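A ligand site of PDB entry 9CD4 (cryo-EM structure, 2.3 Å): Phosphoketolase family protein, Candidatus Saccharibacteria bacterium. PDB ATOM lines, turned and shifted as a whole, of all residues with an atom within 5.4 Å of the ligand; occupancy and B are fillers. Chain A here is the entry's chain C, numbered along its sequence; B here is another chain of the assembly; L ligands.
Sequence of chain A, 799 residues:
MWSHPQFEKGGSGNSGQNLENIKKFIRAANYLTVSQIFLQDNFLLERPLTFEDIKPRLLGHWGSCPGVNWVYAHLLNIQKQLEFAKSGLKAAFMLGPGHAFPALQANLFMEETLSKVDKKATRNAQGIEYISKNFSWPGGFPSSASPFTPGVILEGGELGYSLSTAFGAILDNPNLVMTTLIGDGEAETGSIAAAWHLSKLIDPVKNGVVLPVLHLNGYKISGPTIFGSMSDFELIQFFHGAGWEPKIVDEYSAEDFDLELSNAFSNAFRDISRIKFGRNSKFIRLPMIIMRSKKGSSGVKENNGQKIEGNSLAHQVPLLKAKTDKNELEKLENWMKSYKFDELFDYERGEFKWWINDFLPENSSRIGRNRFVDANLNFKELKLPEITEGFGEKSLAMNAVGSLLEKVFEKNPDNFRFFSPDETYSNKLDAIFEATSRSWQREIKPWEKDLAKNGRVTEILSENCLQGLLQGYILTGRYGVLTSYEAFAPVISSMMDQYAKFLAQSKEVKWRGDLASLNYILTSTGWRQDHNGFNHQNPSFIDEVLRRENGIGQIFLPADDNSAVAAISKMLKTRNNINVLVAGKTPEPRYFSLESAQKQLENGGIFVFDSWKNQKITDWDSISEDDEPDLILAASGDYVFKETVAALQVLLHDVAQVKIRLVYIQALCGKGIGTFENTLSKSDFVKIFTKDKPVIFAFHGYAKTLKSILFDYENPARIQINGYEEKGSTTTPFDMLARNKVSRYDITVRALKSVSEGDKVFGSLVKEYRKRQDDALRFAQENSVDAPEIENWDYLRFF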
ATOM      1  N   HIS A  61     -13.120  31.018 -21.111  1.00  0.00           N
ATOM      2  CA  HIS A  61     -12.956  29.583 -21.267  1.00  0.00           C
ATOM      3  C   HIS A  61     -13.144  29.201 -22.731  1.00  0.00           C
ATOM      4  O   HIS A  61     -13.811  29.904 -23.482  1.00  0.00           O
ATOM      5  CB  HIS A  61     -13.943  28.802 -20.380  1.00  0.00           C
ATOM      6  CG  HIS A  61     -13.822  29.109 -18.918  1.00  0.00           C
ATOM      7  ND1 HIS A  61     -14.239  30.303 -18.375  1.00  0.00           N
ATOM      8  CD2 HIS A  61     -13.332  28.377 -17.887  1.00  0.00           C
ATOM      9  CE1 HIS A  61     -14.013  30.288 -17.069  1.00  0.00           C
ATOM     10  NE2 HIS A  61     -13.468  29.134 -16.747  1.00  0.00           N
ATOM     11  N   GLY A  63     -12.761  25.305 -23.760  1.00  0.00           N
ATOM     12  CA  GLY A  63     -12.819  23.878 -24.035  1.00  0.00           C
ATOM     13  C   GLY A  63     -14.182  23.386 -24.476  1.00  0.00           C
ATOM     14  O   GLY A  63     -14.278  22.474 -25.305  1.00  0.00           O
ATOM     15  N   SER A  64     -15.250  23.961 -23.933  1.00  0.00           N
ATOM     16  CA  SER A  64     -16.604  23.493 -24.210  1.00  0.00           C
ATOM     17  C   SER A  64     -17.288  24.247 -25.347  1.00  0.00           C
ATOM     18  O   SER A  64     -18.407  23.880 -25.724  1.00  0.00           O
ATOM     19  CB  SER A  64     -17.463  23.581 -22.942  1.00  0.00           C
ATOM     20  OG  SER A  64     -17.133  24.729 -22.189  1.00  0.00           O
ATOM     21  N   PRO A  97     -23.217  24.184 -18.992  1.00  0.00           N
ATOM     22  CA  PRO A  97     -21.904  24.791 -18.744  1.00  0.00           C
ATOM     23  C   PRO A  97     -21.891  26.289 -18.993  1.00  0.00           C
ATOM     24  O   PRO A  97     -21.527  26.752 -20.081  1.00  0.00           O
ATOM     25  CB  PRO A  97     -20.987  24.062 -19.737  1.00  0.00           C
ATOM     26  CG  PRO A  97     -21.682  22.782 -20.027  1.00  0.00           C
ATOM     27  CD  PRO A  97     -23.143  23.110 -19.989  1.00  0.00           C
ATOM     28  N   HIS A  99     -19.973  28.543 -18.127  1.00  0.00           N
ATOM     29  CA  HIS A  99     -18.666  29.124 -18.442  1.00  0.00           C
ATOM     30  C   HIS A  99     -18.387  29.171 -19.937  1.00  0.00           C
ATOM     31  O   HIS A  99     -17.427  29.829 -20.345  1.00  0.00           O
ATOM     32  CB  HIS A  99     -17.555  28.351 -17.721  1.00  0.00           C
ATOM     33  CG  HIS A  99     -17.588  26.881 -17.974  1.00  0.00           C
ATOM     34  ND1 HIS A  99     -18.318  26.005 -17.197  1.00  0.00           N
ATOM     35  CD2 HIS A  99     -16.958  26.120 -18.906  1.00  0.00           C
ATOM     36  CE1 HIS A  99     -18.155  24.771 -17.655  1.00  0.00           C
ATOM     37  NE2 HIS A  99     -17.336  24.814 -18.686  1.00  0.00           N
ATOM     38  N   GLY A 157     -23.945  28.820 -13.465  1.00  0.00           N
ATOM     39  CA  GLY A 157     -22.764  29.070 -12.652  1.00  0.00           C
ATOM     40  C   GLY A 157     -22.472  27.933 -11.703  1.00  0.00           C
ATOM     41  O   GLY A 157     -21.448  27.251 -11.838  1.00  0.00           O
ATOM     42  N   GLU A 158     -23.360  27.704 -10.743  1.00  0.00           N
ATOM     43  CA  GLU A 158     -23.264  26.524  -9.899  1.00  0.00           C
ATOM     44  C   GLU A 158     -23.693  25.310 -10.712  1.00  0.00           C
ATOM     45  O   GLU A 158     -24.806  25.262 -11.234  1.00  0.00           O
ATOM     46  CB  GLU A 158     -24.139  26.684  -8.656  1.00  0.00           C
ATOM     47  CG  GLU A 158     -23.891  25.641  -7.584  1.00  0.00           C
ATOM     48  CD  GLU A 158     -24.491  26.030  -6.248  1.00  0.00           C
ATOM     49  OE1 GLU A 158     -24.140  27.108  -5.729  1.00  0.00           O
ATOM     50  OE2 GLU A 158     -25.313  25.257  -5.712  1.00  0.00           O
ATOM     51  N   LEU A 159     -22.795  24.330 -10.839  1.00  0.00           N
ATOM     52  CA  LEU A 159     -23.042  23.189 -11.698  1.00  0.00           C
ATOM     53  C   LEU A 159     -24.186  22.336 -11.171  1.00  0.00           C
ATOM     54  O   LEU A 159     -24.440  22.264  -9.965  1.00  0.00           O
ATOM     55  CB  LEU A 159     -21.778  22.338 -11.831  1.00  0.00           C
ATOM     56  CG  LEU A 159     -20.713  22.898 -12.777  1.00  0.00           C
ATOM     57  CD1 LEU A 159     -19.546  21.932 -12.909  1.00  0.00           C
ATOM     58  CD2 LEU A 159     -21.307  23.227 -14.135  1.00  0.00           C
ATOM     59  N   GLY A 183     -22.636  18.926 -19.078  1.00  0.00           N
ATOM     60  CA  GLY A 183     -21.260  18.473 -19.103  1.00  0.00           C
ATOM     61  C   GLY A 183     -21.059  17.190 -18.323  1.00  0.00           C
ATOM     62  O   GLY A 183     -21.779  16.897 -17.365  1.00  0.00           O
ATOM     63  N   ASP A 184     -20.076  16.400 -18.755  1.00  0.00           N
ATOM     64  CA  ASP A 184     -19.827  15.107 -18.124  1.00  0.00           C
ATOM     65  C   ASP A 184     -19.294  15.256 -16.709  1.00  0.00           C
ATOM     66  O   ASP A 184     -19.601  14.431 -15.840  1.00  0.00           O
ATOM     67  CB  ASP A 184     -18.864  14.279 -18.975  1.00  0.00           C
ATOM     68  CG  ASP A 184     -17.553  14.988 -19.243  1.00  0.00           C
ATOM     69  OD1 ASP A 184     -17.479  16.218 -19.041  1.00  0.00           O
ATOM     70  OD2 ASP A 184     -16.593  14.321 -19.669  1.00  0.00           O
ATOM     71  N   GLY A 185     -18.494  16.289 -16.444  1.00  0.00           N
ATOM     72  CA  GLY A 185     -18.108  16.577 -15.074  1.00  0.00           C
ATOM     73  C   GLY A 185     -19.279  17.034 -14.234  1.00  0.00           C
ATOM     74  O   GLY A 185     -19.417  16.640 -13.075  1.00  0.00           O
ATOM     75  N   GLU A 186     -20.160  17.860 -14.815  1.00  0.00           N
ATOM     76  CA  GLU A 186     -21.353  18.317 -14.121  1.00  0.00           C
ATOM     77  C   GLU A 186     -22.302  17.165 -13.815  1.00  0.00           C
ATOM     78  O   GLU A 186     -23.017  17.201 -12.803  1.00  0.00           O
ATOM     79  CB  GLU A 186     -22.049  19.398 -14.946  1.00  0.00           C
ATOM     80  CG  GLU A 186     -23.418  19.842 -14.458  1.00  0.00           C
ATOM     81  CD  GLU A 186     -24.167  20.646 -15.496  1.00  0.00           C
ATOM     82  OE1 GLU A 186     -23.985  20.386 -16.700  1.00  0.00           O
ATOM     83  OE2 GLU A 186     -24.952  21.541 -15.102  1.00  0.00           O
ATOM     84  N   THR A 189     -22.656  15.357 -10.223  1.00  0.00           N
ATOM     85  CA  THR A 189     -23.340  15.932  -9.071  1.00  0.00           C
ATOM     86  C   THR A 189     -24.568  15.103  -8.702  1.00  0.00           C
ATOM     87  O   THR A 189     -25.065  14.300  -9.485  1.00  0.00           O
ATOM     88  CB  THR A 189     -23.746  17.380  -9.348  1.00  0.00           C
ATOM     89  OG1 THR A 189     -24.330  17.472 -10.649  1.00  0.00           O
ATOM     90  CG2 THR A 189     -22.533  18.299  -9.268  1.00  0.00           C
ATOM     91  N   HIS A 215     -22.255  16.283 -23.073  1.00  0.00           N
ATOM     92  CA  HIS A 215     -20.987  16.684 -23.660  1.00  0.00           C
ATOM     93  C   HIS A 215     -19.874  15.904 -22.980  1.00  0.00           C
ATOM     94  O   HIS A 215     -19.341  16.304 -21.945  1.00  0.00           O
ATOM     95  CB  HIS A 215     -20.778  18.185 -23.513  1.00  0.00           C
ATOM     96  CG  HIS A 215     -19.730  18.752 -24.419  1.00  0.00           C
ATOM     97  ND1 HIS A 215     -19.347  20.077 -24.389  1.00  0.00           N
ATOM     98  CD2 HIS A 215     -18.984  18.173 -25.388  1.00  0.00           C
ATOM     99  CE1 HIS A 215     -18.413  20.289 -25.296  1.00  0.00           C
ATOM    100  NE2 HIS A 215     -18.174  19.147 -25.919  1.00  0.00           N
ATOM    101  N   ASN A 217     -16.637  15.353 -23.210  1.00  0.00           N
ATOM    102  CA  ASN A 217     -15.279  15.707 -23.610  1.00  0.00           C
ATOM    103  C   ASN A 217     -14.235  14.874 -22.878  1.00  0.00           C
ATOM    104  O   ASN A 217     -13.167  14.603 -23.434  1.00  0.00           O
ATOM    105  CB  ASN A 217     -15.017  17.202 -23.391  1.00  0.00           C
ATOM    106  CG  ASN A 217     -15.576  17.702 -22.082  1.00  0.00           C
ATOM    107  OD1 ASN A 217     -15.335  17.118 -21.025  1.00  0.00           O
ATOM    108  ND2 ASN A 217     -16.312  18.803 -22.126  1.00  0.00           N
ATOM    109  N   TYR A 219     -12.851  15.495 -19.668  1.00  0.00           N
ATOM    110  CA  TYR A 219     -11.963  16.146 -18.714  1.00  0.00           C
ATOM    111  C   TYR A 219     -12.716  17.206 -17.916  1.00  0.00           C
ATOM    112  O   TYR A 219     -13.599  17.901 -18.428  1.00  0.00           O
ATOM    113  CB  TYR A 219     -10.751  16.777 -19.412  1.00  0.00           C
ATOM    114  CG  TYR A 219      -9.787  15.757 -19.973  1.00  0.00           C
ATOM    115  CD1 TYR A 219      -8.698  15.307 -19.241  1.00  0.00           C
ATOM    116  CD2 TYR A 219      -9.974  15.234 -21.259  1.00  0.00           C
ATOM    117  CE1 TYR A 219      -7.824  14.374 -19.749  1.00  0.00           C
ATOM    118  CE2 TYR A 219      -9.101  14.293 -21.773  1.00  0.00           C
ATOM    119  CZ  TYR A 219      -8.033  13.871 -21.012  1.00  0.00           C
ATOM    120  OH  TYR A 219      -7.166  12.935 -21.532  1.00  0.00           O
ATOM    121  N   LYS A 220     -12.356  17.292 -16.645  1.00  0.00           N
ATOM    122  CA  LYS A 220     -12.795  18.353 -15.740  1.00  0.00           C
ATOM    123  C   LYS A 220     -11.785  19.498 -15.813  1.00  0.00           C
ATOM    124  O   LYS A 220     -11.052  19.568 -16.812  1.00  0.00           O
ATOM    125  CB  LYS A 220     -13.015  17.774 -14.345  1.00  0.00           C
ATOM    126  CG  LYS A 220     -14.221  16.869 -14.234  1.00  0.00           C
ATOM    127  CD  LYS A 220     -13.915  15.632 -13.401  1.00  0.00           C
ATOM    128  CE  LYS A 220     -13.771  15.974 -11.935  1.00  0.00           C
ATOM    129  NZ  LYS A 220     -13.513  14.760 -11.114  1.00  0.00           N
ATOM    130  N   ILE A 221     -11.750  20.422 -14.853  1.00  0.00           N
ATOM    131  CA  ILE A 221     -10.774  21.506 -14.850  1.00  0.00           C
ATOM    132  C   ILE A 221      -9.349  20.969 -14.929  1.00  0.00           C
ATOM    133  O   ILE A 221      -8.551  21.419 -15.749  1.00  0.00           O
ATOM    134  CB  ILE A 221     -10.959  22.395 -13.601  1.00  0.00           C
ATOM    135  CG1 ILE A 221     -12.282  23.166 -13.672  1.00  0.00           C
ATOM    136  CG2 ILE A 221      -9.790  23.352 -13.439  1.00  0.00           C
ATOM    137  CD1 ILE A 221     -12.473  24.142 -12.535  1.00  0.00           C
ATOM    138  N   THR A 225     -12.800  12.582 -16.088  1.00  0.00           N
ATOM    139  CA  THR A 225     -14.126  12.470 -15.494  1.00  0.00           C
ATOM    140  C   THR A 225     -14.478  11.024 -15.211  1.00  0.00           C
ATOM    141  O   THR A 225     -13.880  10.092 -15.749  1.00  0.00           O
ATOM    142  CB  THR A 225     -15.186  13.084 -16.418  1.00  0.00           C
ATOM    143  OG1 THR A 225     -15.365  12.242 -17.559  1.00  0.00           O
ATOM    144  CG2 THR A 225     -14.766  14.459 -16.870  1.00  0.00           C
ATOM    145  N   LYS A 295     -11.631  17.799 -26.088  1.00  0.00           N
ATOM    146  CA  LYS A 295     -11.845  19.064 -25.411  1.00  0.00           C
ATOM    147  C   LYS A 295     -11.004  20.161 -26.050  1.00  0.00           C
ATOM    148  O   LYS A 295      -9.805  19.989 -26.282  1.00  0.00           O
ATOM    149  CB  LYS A 295     -11.497  18.931 -23.927  1.00  0.00           C
ATOM    150  CG  LYS A 295     -11.629  20.228 -23.146  1.00  0.00           C
ATOM    151  CD  LYS A 295     -11.944  19.963 -21.681  1.00  0.00           C
ATOM    152  CE  LYS A 295     -12.006  21.257 -20.897  1.00  0.00           C
ATOM    153  NZ  LYS A 295     -12.837  21.121 -19.669  1.00  0.00           N
ATOM    154  N   HIS A 315      -9.059  23.955 -20.620  1.00  0.00           N
ATOM    155  CA  HIS A 315     -10.244  24.440 -19.913  1.00  0.00           C
ATOM    156  C   HIS A 315     -10.332  25.959 -19.946  1.00  0.00           C
ATOM    157  O   HIS A 315     -11.305  26.534 -20.434  1.00  0.00           O
ATOM    158  CB  HIS A 315     -10.229  23.926 -18.475  1.00  0.00           C
ATOM    159  CG  HIS A 315     -11.466  24.271 -17.703  1.00  0.00           C
ATOM    160  ND1 HIS A 315     -12.657  23.597 -17.868  1.00  0.00           N
ATOM    161  CD2 HIS A 315     -11.699  25.214 -16.749  1.00  0.00           C
ATOM    162  CE1 HIS A 315     -13.563  24.105 -17.048  1.00  0.00           C
ATOM    163  NE2 HIS A 315     -13.010  25.092 -16.369  1.00  0.00           N
ATOM    164  N   PRO B 421     -12.848  18.873  -4.573  1.00  0.00           N
ATOM    165  CA  PRO B 421     -13.692  18.651  -5.764  1.00  0.00           C
ATOM    166  C   PRO B 421     -13.035  19.128  -7.051  1.00  0.00           C
ATOM    167  O   PRO B 421     -13.517  20.061  -7.724  1.00  0.00           O
ATOM    168  CB  PRO B 421     -14.955  19.433  -5.415  1.00  0.00           C
ATOM    169  CG  PRO B 421     -14.451  20.582  -4.584  1.00  0.00           C
ATOM    170  CD  PRO B 421     -13.191  20.118  -3.886  1.00  0.00           C
ATOM    171  N   ASP B 422     -11.929  18.472  -7.412  1.00  0.00           N
ATOM    172  CA  ASP B 422     -11.155  18.777  -8.628  1.00  0.00           C
ATOM    173  C   ASP B 422     -10.720  20.242  -8.664  1.00  0.00           C
ATOM    174  O   ASP B 422     -10.866  20.930  -9.676  1.00  0.00           O
ATOM    175  CB  ASP B 422     -11.940  18.388  -9.883  1.00  0.00           C
ATOM    176  CG  ASP B 422     -11.046  18.188 -11.091  1.00  0.00           C
ATOM    177  OD1 ASP B 422     -10.352  17.156 -11.150  1.00  0.00           O
ATOM    178  OD2 ASP B 422     -11.048  19.068 -11.976  1.00  0.00           O
ATOM    179  N   GLU B 423     -10.195  20.723  -7.538  1.00  0.00           N
ATOM    180  CA  GLU B 423      -9.862  22.131  -7.419  1.00  0.00           C
ATOM    181  C   GLU B 423      -8.519  22.390  -6.748  1.00  0.00           C
ATOM    182  O   GLU B 423      -8.212  23.547  -6.441  1.00  0.00           O
ATOM    183  CB  GLU B 423     -10.954  22.870  -6.648  1.00  0.00           C
ATOM    184  CG  GLU B 423     -12.091  23.394  -7.505  1.00  0.00           C
ATOM    185  CD  GLU B 423     -13.403  23.461  -6.750  1.00  0.00           C
ATOM    186  OE1 GLU B 423     -13.465  24.180  -5.725  1.00  0.00           O
ATOM    187  OE2 GLU B 423     -14.370  22.800  -7.177  1.00  0.00           O
ATOM    188  N   LEU B 461     -16.558  15.622  -8.266  1.00  0.00           N
ATOM    189  CA  LEU B 461     -17.268  16.895  -8.253  1.00  0.00           C
ATOM    190  C   LEU B 461     -18.443  16.907  -7.287  1.00  0.00           C
ATOM    191  O   LEU B 461     -19.009  17.976  -7.036  1.00  0.00           O
ATOM    192  CB  LEU B 461     -17.745  17.238  -9.663  1.00  0.00           C
ATOM    193  CG  LEU B 461     -17.266  18.590 -10.200  1.00  0.00           C
ATOM    194  CD1 LEU B 461     -17.257  18.599 -11.710  1.00  0.00           C
ATOM    195  CD2 LEU B 461     -18.132  19.718  -9.664  1.00  0.00           C
ATOM    196  N   GLU B 463     -19.840  17.265  -3.905  1.00  0.00           N
ATOM    197  CA  GLU B 463     -19.417  17.719  -2.583  1.00  0.00           C
ATOM    198  C   GLU B 463     -20.012  16.865  -1.480  1.00  0.00           C
ATOM    199  O   GLU B 463     -19.398  16.715  -0.413  1.00  0.00           O
ATOM    200  CB  GLU B 463     -19.800  19.189  -2.389  1.00  0.00           C
ATOM    201  CG  GLU B 463     -18.991  20.163  -3.226  1.00  0.00           C
ATOM    202  CD  GLU B 463     -19.587  20.403  -4.600  1.00  0.00           C
ATOM    203  OE1 GLU B 463     -20.580  19.735  -4.936  1.00  0.00           O
ATOM    204  OE2 GLU B 463     -19.051  21.240  -5.342  1.00  0.00           O
ATOM    205  N   TYR B 485     -14.049  25.731  -2.908  1.00  0.00           N
ATOM    206  CA  TYR B 485     -14.383  27.127  -3.104  1.00  0.00           C
ATOM    207  C   TYR B 485     -15.317  27.595  -1.992  1.00  0.00           C
ATOM    208  O   TYR B 485     -16.030  26.805  -1.372  1.00  0.00           O
ATOM    209  CB  TYR B 485     -15.059  27.348  -4.454  1.00  0.00           C
ATOM    210  CG  TYR B 485     -14.141  27.241  -5.651  1.00  0.00           C
ATOM    211  CD1 TYR B 485     -12.765  27.413  -5.515  1.00  0.00           C
ATOM    212  CD2 TYR B 485     -14.650  26.996  -6.914  1.00  0.00           C
ATOM    213  CE1 TYR B 485     -11.935  27.329  -6.611  1.00  0.00           C
ATOM    214  CE2 TYR B 485     -13.827  26.908  -8.021  1.00  0.00           C
ATOM    215  CZ  TYR B 485     -12.459  27.076  -7.864  1.00  0.00           C
ATOM    216  OH  TYR B 485     -11.637  26.987  -8.954  1.00  0.00           O
ATOM    217  N   PHE B 488     -19.387  27.381  -3.282  1.00  0.00           N
ATOM    218  CA  PHE B 488     -20.075  26.107  -3.404  1.00  0.00           C
ATOM    219  C   PHE B 488     -20.053  25.298  -2.109  1.00  0.00           C
ATOM    220  O   PHE B 488     -20.487  24.137  -2.104  1.00  0.00           O
ATOM    221  CB  PHE B 488     -19.474  25.298  -4.549  1.00  0.00           C
ATOM    222  CG  PHE B 488     -19.407  26.050  -5.837  1.00  0.00           C
ATOM    223  CD1 PHE B 488     -20.548  26.618  -6.379  1.00  0.00           C
ATOM    224  CD2 PHE B 488     -18.202  26.205  -6.515  1.00  0.00           C
ATOM    225  CE1 PHE B 488     -20.495  27.320  -7.572  1.00  0.00           C
ATOM    226  CE2 PHE B 488     -18.141  26.902  -7.702  1.00  0.00           C
ATOM    227  CZ  PHE B 488     -19.284  27.462  -8.233  1.00  0.00           C
ATOM    228  N   ASN B 532     -14.799  34.311 -13.441  1.00  0.00           N
ATOM    229  CA  ASN B 532     -16.198  33.995 -13.203  1.00  0.00           C
ATOM    230  C   ASN B 532     -16.928  35.252 -12.735  1.00  0.00           C
ATOM    231  O   ASN B 532     -16.304  36.262 -12.375  1.00  0.00           O
ATOM    232  CB  ASN B 532     -16.355  32.869 -12.182  1.00  0.00           C
ATOM    233  CG  ASN B 532     -15.564  31.634 -12.565  1.00  0.00           C
ATOM    234  OD1 ASN B 532     -15.762  31.059 -13.641  1.00  0.00           O
ATOM    235  ND2 ASN B 532     -14.649  31.224 -11.689  1.00  0.00           N
ATOM    236  N   HIS B 536     -20.346  33.137  -8.378  1.00  0.00           N
ATOM    237  CA  HIS B 536     -19.249  32.617  -7.575  1.00  0.00           C
ATOM    238  C   HIS B 536     -18.959  33.483  -6.352  1.00  0.00           C
ATOM    239  O   HIS B 536     -17.814  33.541  -5.892  1.00  0.00           O
ATOM    240  CB  HIS B 536     -17.994  32.452  -8.430  1.00  0.00           C
ATOM    241  CG  HIS B 536     -18.082  31.375  -9.452  1.00  0.00           C
ATOM    242  ND1 HIS B 536     -18.985  31.404 -10.492  1.00  0.00           N
ATOM    243  CD2 HIS B 536     -17.383  30.220  -9.597  1.00  0.00           C
ATOM    244  CE1 HIS B 536     -18.838  30.322 -11.238  1.00  0.00           C
ATOM    245  NE2 HIS B 536     -17.873  29.590 -10.712  1.00  0.00           N
HETATM  246  N1  LIG L   1     -18.420  22.858  -8.150  1.00  0.00           N
HETATM  247  C1  LIG L   1     -19.671  23.167  -8.572  1.00  0.00           C
HETATM  248  C2  LIG L   1     -20.889  22.518  -7.915  1.00  0.00           C
HETATM  249  N2  LIG L   1     -19.844  24.049  -9.586  1.00  0.00           N
HETATM  250  C3  LIG L   1     -18.802  24.610 -10.163  1.00  0.00           C
HETATM  251  N3  LIG L   1     -19.012  25.554 -11.239  1.00  0.00           N
HETATM  252  C4  LIG L   1     -17.544  24.305  -9.746  1.00  0.00           C
HETATM  253  C5  LIG L   1     -17.379  23.420  -8.727  1.00  0.00           C
HETATM  254  C6  LIG L   1     -16.312  24.945 -10.391  1.00  0.00           C
HETATM  255  N4  LIG L   1     -16.193  24.530 -11.786  1.00  0.00           N
HETATM  256  C7  LIG L   1     -16.356  25.340 -12.936  1.00  0.00           C
HETATM  257  S1  LIG L   1     -16.135  24.463 -14.183  1.00  0.00           S
HETATM  258  C8  LIG L   1     -15.835  23.057 -13.700  1.00  0.00           C
HETATM  259  C9  LIG L   1     -15.861  23.073 -12.271  1.00  0.00           C
HETATM  260  C10 LIG L   1     -15.605  21.863 -11.374  1.00  0.00           C
HETATM  261  C11 LIG L   1     -15.546  21.845 -14.573  1.00  0.00           C
HETATM  262  C12 LIG L   1     -16.791  21.554 -15.415  1.00  0.00           C
HETATM  263  O1  LIG L   1     -16.815  20.203 -15.754  1.00  0.00           O
HETATM  264  P1  LIG L   1     -17.347  19.834 -17.262  1.00  0.00           P
HETATM  265  O2  LIG L   1     -17.114  21.157 -18.211  1.00  0.00           O
HETATM  266  O3  LIG L   1     -16.583  18.645 -17.800  1.00  0.00           O
HETATM  267  O4  LIG L   1     -18.817  19.495 -17.202  1.00  0.00           O
HETATM  268  P2  LIG L   1     -16.643  21.131 -19.794  1.00  0.00           P
HETATM  269  O5  LIG L   1     -15.552  20.111 -20.002  1.00  0.00           O
HETATM  270  O6  LIG L   1     -17.817  20.790 -20.670  1.00  0.00           O
HETATM  271  O7  LIG L   1     -16.114  22.496 -20.155  1.00  0.00           O
HETATM  272  C13 LIG L   1     -16.692  26.842 -12.976  1.00  0.00           C
HETATM  273  O8  LIG L   1     -17.490  27.297 -12.235  1.00  0.00           O
HETATM  274  C14 LIG L   1     -15.972  27.743 -13.977  1.00  0.00           C
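An oxygen (O3) of the ligand lies close to the backbone carbonyl oxygen (O) of Tyr 219 (3.1 Å).
OE2 of Glu 463 of chain B sits close to N1 of the ligand, 3.3 Å away.
His 61 touches the ligand.
CA of Gly 183 touches O4 of the ligand, 3.3 Å away.
Ile 221 touches the ligand (CG1 to C8, 3.6 Å).
His 315 touches the ligand.
OE2 of Glu 423 of chain B touches C5 of the ligand, at 3.4 Å.
CD2 of Leu 461 of chain B touches N1 of the ligand, at 3.5 Å.
Tyr 485 of chain B touches the ligand.
CE2 of Phe 488 of chain B touches C4 of the ligand, at 3.4 Å.
Asn 532 of chain B touches the ligand (OD1 to C14, 3.3 Å).
Hydrophobic or aromatic side chains within 4 Å of the ligand: His 99, Leu 159, Ile 221, His 315, Leu 461 of chain B, Tyr 485 of chain B, Phe 488 of chain B and His 536 of chain B.
21 residues have an atom within 4 Å of the ligand: His 61, Ser 64, His 99, Gly 157, Leu 159, Gly 183, Asp 184, Gly 185, Glu 186, Asn 217, Tyr 219, Ile 221, Lys 295, His 315, Glu 423 of chain B, Leu 461 of chain B, Glu 463 of chain B, Tyr 485 of chain B, Phe 488 of chain B, Asn 532 of chain B and His 536 of chain B.
The side-chain amide nitrogen (ND2) of Asn 217 lies within hydrogen-bond range of an oxygen (O5) of the ligand (2.6 Å).
O8 of the ligand sits at hydrogen-bond distance from NE2 of His 536 of chain B, at 2.8 Å.
OD1 of Asp 184 lies close to O3 of the ligand (2.9 Å).
The side-chain amino group (NZ) of Lys 295 lies within salt-bridge range of an oxygen (O5) of the ligand.
A ring nitrogen (NE2) of His 99 is in hydrogen-bond range of an oxygen (O7) of the ligand (3.0 Å).
The backbone carbonyl oxygen (O) of Gly 157 lies within hydrogen-bond range of a nitrogen (N3) of the ligand (3.0 Å).
The side-chain hydroxyl (OG) of Ser 64 sits at hydrogen-bond distance from an oxygen (O7) of the ligand (3.2 Å).
N of Glu 186 sits at hydrogen-bond distance from O4 of the ligand, at 3.2 Å.
The backbone NH (N) of Leu 159 sits at hydrogen-bond distance from a nitrogen (N2) of the ligand (3.2 Å).
The backbone NH of Gly 185 is in hydrogen-bond range of an oxygen (O4) of the ligand, 3.3 Å away.
OD1 of Asp 184 sits close to OD1 of Asn 217 (3.1 Å).
OD1 of Asn 217 lies close to O of Tyr 219.
The backbone NH of Asp 184 sits at hydrogen-bond distance from the backbone carbonyl oxygen of His 215, 3.3 Å away.
The side-chain carboxylate of Asp 184 lies within hydrogen-bond range of the side-chain hydroxyl of Thr 225 (3.2 Å).
OE1 of Glu 186 lies within hydrogen-bond range of N of Gly 183.
OG1 of Thr 189 is in hydrogen-bond range of O of Glu 186 (2.5 Å).
The side-chain carboxylate of Glu 423 of chain B sits close to the backbone NH of Tyr 485 of chain B, 3.3 Å away.
The backbone NH (N) of Ile 221 lies within hydrogen-bond range of the side-chain carboxylate (OD2) of Asp 422 of chain B (3.3 Å).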
